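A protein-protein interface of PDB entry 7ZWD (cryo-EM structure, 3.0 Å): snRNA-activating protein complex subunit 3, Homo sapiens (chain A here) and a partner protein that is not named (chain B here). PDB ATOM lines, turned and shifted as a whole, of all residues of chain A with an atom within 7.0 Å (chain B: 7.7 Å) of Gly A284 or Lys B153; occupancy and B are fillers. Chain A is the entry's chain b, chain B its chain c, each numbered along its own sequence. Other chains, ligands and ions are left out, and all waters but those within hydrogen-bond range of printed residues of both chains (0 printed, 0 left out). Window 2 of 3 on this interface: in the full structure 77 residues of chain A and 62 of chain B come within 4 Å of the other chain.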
ATOM      1  N   TRP A 277      33.417   1.156   8.254  1.00  0.00           N
ATOM      2  CA  TRP A 277      32.951   0.230   7.234  1.00  0.00           C
ATOM      3  C   TRP A 277      31.494   0.458   6.881  1.00  0.00           C
ATOM      4  O   TRP A 277      31.084   0.135   5.766  1.00  0.00           O
ATOM      5  CB  TRP A 277      33.170  -1.199   7.720  1.00  0.00           C
ATOM      6  CG  TRP A 277      32.360  -2.255   7.057  1.00  0.00           C
ATOM      7  CD1 TRP A 277      32.678  -2.935   5.930  1.00  0.00           C
ATOM      8  CD2 TRP A 277      31.120  -2.798   7.514  1.00  0.00           C
ATOM      9  NE1 TRP A 277      31.707  -3.855   5.639  1.00  0.00           N
ATOM     10  CE2 TRP A 277      30.740  -3.793   6.604  1.00  0.00           C
ATOM     11  CE3 TRP A 277      30.291  -2.534   8.602  1.00  0.00           C
ATOM     12  CZ2 TRP A 277      29.565  -4.513   6.740  1.00  0.00           C
ATOM     13  CZ3 TRP A 277      29.131  -3.253   8.736  1.00  0.00           C
ATOM     14  CH2 TRP A 277      28.776  -4.227   7.812  1.00  0.00           C
ATOM     15  N   SER A 278      30.712   1.009   7.798  1.00  0.00           N
ATOM     16  CA  SER A 278      29.330   1.344   7.492  1.00  0.00           C
ATOM     17  C   SER A 278      29.160   2.773   7.005  1.00  0.00           C
ATOM     18  O   SER A 278      28.181   3.066   6.312  1.00  0.00           O
ATOM     19  CB  SER A 278      28.452   1.120   8.719  1.00  0.00           C
ATOM     20  OG  SER A 278      27.119   1.499   8.445  1.00  0.00           O
ATOM     21  N   HIS A 281      29.821   2.792   1.618  1.00  0.00           N
ATOM     22  CA  HIS A 281      28.661   2.320   0.871  1.00  0.00           C
ATOM     23  C   HIS A 281      27.598   1.747   1.798  1.00  0.00           C
ATOM     24  O   HIS A 281      27.925   1.033   2.747  1.00  0.00           O
ATOM     25  CB  HIS A 281      29.094   1.250  -0.130  1.00  0.00           C
ATOM     26  CG  HIS A 281      30.205   1.685  -1.029  1.00  0.00           C
ATOM     27  ND1 HIS A 281      31.531   1.471  -0.723  1.00  0.00           N
ATOM     28  CD2 HIS A 281      30.192   2.344  -2.210  1.00  0.00           C
ATOM     29  CE1 HIS A 281      32.288   1.968  -1.684  1.00  0.00           C
ATOM     30  NE2 HIS A 281      31.501   2.504  -2.598  1.00  0.00           N
ATOM     31  N   ASP A 282      26.334   2.089   1.558  1.00  0.00           N
ATOM     32  CA  ASP A 282      25.221   1.664   2.402  1.00  0.00           C
ATOM     33  C   ASP A 282      25.269   0.149   2.511  1.00  0.00           C
ATOM     34  O   ASP A 282      25.467  -0.542   1.509  1.00  0.00           O
ATOM     35  CB  ASP A 282      23.882   2.130   1.830  1.00  0.00           C
ATOM     36  CG  ASP A 282      22.715   1.826   2.751  1.00  0.00           C
ATOM     37  OD1 ASP A 282      22.935   1.242   3.833  1.00  0.00           O
ATOM     38  OD2 ASP A 282      21.569   2.172   2.392  1.00  0.00           O
ATOM     39  N   ARG A 283      25.088  -0.365   3.722  1.00  0.00           N
ATOM     40  CA  ARG A 283      25.276  -1.783   3.976  1.00  0.00           C
ATOM     41  C   ARG A 283      24.136  -2.340   4.806  1.00  0.00           C
ATOM     42  O   ARG A 283      24.313  -3.286   5.576  1.00  0.00           O
ATOM     43  CB  ARG A 283      26.609  -2.029   4.667  1.00  0.00           C
ATOM     44  CG  ARG A 283      27.779  -1.856   3.745  1.00  0.00           C
ATOM     45  CD  ARG A 283      29.070  -1.978   4.485  1.00  0.00           C
ATOM     46  NE  ARG A 283      30.173  -2.359   3.614  1.00  0.00           N
ATOM     47  CZ  ARG A 283      30.948  -1.505   2.964  1.00  0.00           C
ATOM     48  NH1 ARG A 283      30.748  -0.203   3.076  1.00  0.00           N
ATOM     49  NH2 ARG A 283      31.928  -1.956   2.204  1.00  0.00           N
ATOM     50  N   GLY A 284      22.944  -1.786   4.639  1.00  0.00           N
ATOM     51  CA  GLY A 284      21.848  -2.243   5.460  1.00  0.00           C
ATOM     52  C   GLY A 284      21.826  -1.541   6.807  1.00  0.00           C
ATOM     53  O   GLY A 284      20.873  -0.853   7.175  1.00  0.00           O
ATOM     54  N   TYR A 285      22.909  -1.732   7.546  1.00  0.00           N
ATOM     55  CA  TYR A 285      23.095  -1.082   8.846  1.00  0.00           C
ATOM     56  C   TYR A 285      23.097   0.431   8.632  1.00  0.00           C
ATOM     57  O   TYR A 285      23.322   0.914   7.516  1.00  0.00           O
ATOM     58  CB  TYR A 285      24.342  -1.620   9.500  1.00  0.00           C
ATOM     59  CG  TYR A 285      24.284  -3.097   9.750  1.00  0.00           C
ATOM     60  CD1 TYR A 285      23.601  -3.602  10.835  1.00  0.00           C
ATOM     61  CD2 TYR A 285      24.905  -3.987   8.901  1.00  0.00           C
ATOM     62  CE1 TYR A 285      23.540  -4.945  11.071  1.00  0.00           C
ATOM     63  CE2 TYR A 285      24.846  -5.335   9.128  1.00  0.00           C
ATOM     64  CZ  TYR A 285      24.161  -5.809  10.216  1.00  0.00           C
ATOM     65  OH  TYR A 285      24.092  -7.158  10.461  1.00  0.00           O
ATOM     66  N   GLY A 286      22.858   1.188   9.693  1.00  0.00           N
ATOM     67  CA  GLY A 286      22.898   2.632   9.638  1.00  0.00           C
ATOM     68  C   GLY A 286      22.667   3.257  11.000  1.00  0.00           C
ATOM     69  O   GLY A 286      22.052   2.678  11.898  1.00  0.00           O
ATOM     70  N   PHE B 150      28.105  -8.571  11.966  1.00  0.00           N
ATOM     71  CA  PHE B 150      27.763  -7.571  10.971  1.00  0.00           C
ATOM     72  C   PHE B 150      28.110  -8.094   9.594  1.00  0.00           C
ATOM     73  O   PHE B 150      29.137  -8.746   9.409  1.00  0.00           O
ATOM     74  CB  PHE B 150      28.512  -6.272  11.230  1.00  0.00           C
ATOM     75  CG  PHE B 150      28.207  -5.671  12.546  1.00  0.00           C
ATOM     76  CD1 PHE B 150      27.090  -4.896  12.717  1.00  0.00           C
ATOM     77  CD2 PHE B 150      29.029  -5.896  13.623  1.00  0.00           C
ATOM     78  CE1 PHE B 150      26.810  -4.351  13.928  1.00  0.00           C
ATOM     79  CE2 PHE B 150      28.747  -5.352  14.834  1.00  0.00           C
ATOM     80  CZ  PHE B 150      27.638  -4.581  14.988  1.00  0.00           C
ATOM     81  N   LYS B 151      27.251  -7.805   8.627  1.00  0.00           N
ATOM     82  CA  LYS B 151      27.508  -8.250   7.272  1.00  0.00           C
ATOM     83  C   LYS B 151      26.624  -7.466   6.320  1.00  0.00           C
ATOM     84  O   LYS B 151      25.491  -7.125   6.658  1.00  0.00           O
ATOM     85  CB  LYS B 151      27.270  -9.755   7.132  1.00  0.00           C
ATOM     86  CG  LYS B 151      25.942 -10.224   7.646  1.00  0.00           C
ATOM     87  CD  LYS B 151      25.826 -11.732   7.544  1.00  0.00           C
ATOM     88  CE  LYS B 151      26.737 -12.420   8.536  1.00  0.00           C
ATOM     89  NZ  LYS B 151      26.485 -13.875   8.663  1.00  0.00           N
ATOM     90  N   ASP B 152      27.165  -7.176   5.141  1.00  0.00           N
ATOM     91  CA  ASP B 152      26.427  -6.470   4.109  1.00  0.00           C
ATOM     92  C   ASP B 152      25.093  -7.143   3.838  1.00  0.00           C
ATOM     93  O   ASP B 152      24.971  -8.368   3.868  1.00  0.00           O
ATOM     94  CB  ASP B 152      27.227  -6.446   2.811  1.00  0.00           C
ATOM     95  CG  ASP B 152      28.485  -5.628   2.911  1.00  0.00           C
ATOM     96  OD1 ASP B 152      28.472  -4.469   2.460  1.00  0.00           O
ATOM     97  OD2 ASP B 152      29.487  -6.138   3.447  1.00  0.00           O
ATOM     98  N   LYS B 153      24.083  -6.330   3.559  1.00  0.00           N
ATOM     99  CA  LYS B 153      22.863  -6.838   2.958  1.00  0.00           C
ATOM    100  C   LYS B 153      23.029  -7.041   1.464  1.00  0.00           C
ATOM    101  O   LYS B 153      22.102  -7.513   0.802  1.00  0.00           O
ATOM    102  CB  LYS B 153      21.693  -5.893   3.232  1.00  0.00           C
ATOM    103  CG  LYS B 153      21.353  -5.705   4.706  1.00  0.00           C
ATOM    104  CD  LYS B 153      21.618  -6.956   5.533  1.00  0.00           C
ATOM    105  CE  LYS B 153      20.816  -6.936   6.821  1.00  0.00           C
ATOM    106  NZ  LYS B 153      20.873  -5.611   7.495  1.00  0.00           N
ATOM    107  N   VAL B 154      24.201  -6.707   0.931  1.00  0.00           N
ATOM    108  CA  VAL B 154      24.489  -6.821  -0.490  1.00  0.00           C
ATOM    109  C   VAL B 154      25.361  -8.041  -0.725  1.00  0.00           C
ATOM    110  O   VAL B 154      24.953  -8.992  -1.398  1.00  0.00           O
ATOM    111  CB  VAL B 154      25.184  -5.550  -1.003  1.00  0.00           C
ATOM    112  CG1 VAL B 154      25.442  -5.652  -2.488  1.00  0.00           C
ATOM    113  CG2 VAL B 154      24.343  -4.329  -0.678  1.00  0.00           C
ATOM    114  N   THR B 155      26.559  -8.027  -0.151  1.00  0.00           N
ATOM    115  CA  THR B 155      27.514  -9.105  -0.348  1.00  0.00           C
ATOM    116  C   THR B 155      27.509 -10.110   0.788  1.00  0.00           C
ATOM    117  O   THR B 155      27.803 -11.287   0.562  1.00  0.00           O
ATOM    118  CB  THR B 155      28.919  -8.533  -0.504  1.00  0.00           C
ATOM    119  OG1 THR B 155      29.416  -8.157   0.783  1.00  0.00           O
ATOM    120  CG2 THR B 155      28.891  -7.308  -1.397  1.00  0.00           C
ATOM    121  N   GLY B 156      27.193  -9.676   2.000  1.00  0.00           N
ATOM    122  CA  GLY B 156      27.136 -10.590   3.121  1.00  0.00           C
ATOM    123  C   GLY B 156      28.472 -10.890   3.760  1.00  0.00           C
ATOM    124  O   GLY B 156      28.656 -11.977   4.318  1.00  0.00           O
ATOM    125  N   VAL B 157      29.415  -9.956   3.695  1.00  0.00           N
ATOM    126  CA  VAL B 157      30.723 -10.117   4.315  1.00  0.00           C
ATOM    127  C   VAL B 157      30.855  -9.104   5.439  1.00  0.00           C
ATOM    128  O   VAL B 157      30.323  -7.992   5.354  1.00  0.00           O
ATOM    129  CB  VAL B 157      31.863  -9.961   3.292  1.00  0.00           C
ATOM    130  CG1 VAL B 157      31.709 -10.978   2.193  1.00  0.00           C
ATOM    131  CG2 VAL B 157      31.880  -8.566   2.721  1.00  0.00           C
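Of the printed residues of chain B, Trp A277 touches Phe B150, Lys B151, Asp B152 and Val B157.
Gly A284 touches just one residue of chain B: Lys B153.
Printed residues of chain A within 4 Å of Phe B150: Trp A277 (3.96 Å) and Tyr A285 (3.7 Å).
Of the printed residues of chain A, Lys B151 touches Trp A277 (3.97 Å) and Tyr A285 (3.1 Å).
Of the printed residues of chain A, Asp B152 touches Trp A277 (3.7 Å) and Arg A283 (2.9 Å).
Lys B153 touches two residues of chain A.
Of the printed residues of chain A, Val B157 touches Trp A277.
The nearest residue of chain A that does not touch Lys B153 is Tyr A285 (4.3 Å).
The nearest printed residue of chain A that does not touch Val B157 is Arg A283 (5.9 Å).
Among the printed residues, merely in contact across the chains: Trp A277 with Phe B150, Trp A277 with Lys B151, Trp A277 with Asp B152, Trp A277 with Val B157, Arg A283 with Lys B153, Gly A284 with Lys B153, Tyr A285 with Phe B150 and Tyr A285 with Lys B151.
Printed residues of chain A that touch a printed residue of chain B: Trp A277, Arg A283, Gly A284 and Tyr A285.
Hydrophobic or aromatic side chains of chain A within 4 Å of the printed part of chain B: Trp A277 and Tyr A285.
Among the printed residues, 9 pairs touch across the chains.
The side-chain carboxylate (OD1) of Asp B152 is in salt-bridge range of the guanidinium group (NE) of Arg A283.
O of Trp A277 is in hydrogen-bond range of NH1 of Arg A283 (2.7 Å).
The backbone carbonyl oxygen of His A281 lies close to the guanidinium group of Arg A283.
The side-chain carboxylate (OD1) of Asp A282 sits at hydrogen-bond distance from the backbone NH (N) of Gly A284, 3.1 Å away.
The side-chain carboxylate (OD2) of Asp B152 sits at hydrogen-bond distance from the side-chain hydroxyl (OG1) of Thr B155 (3.3 Å).
The backbone carbonyl oxygen of Val B157 sits at hydrogen-bond distance from the backbone NH of Asp B152 (3.3 Å).
The backbone NH (N) of Val B157 lies close to the side-chain hydroxyl (OG1) of Thr B155, 3.4 Å away.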
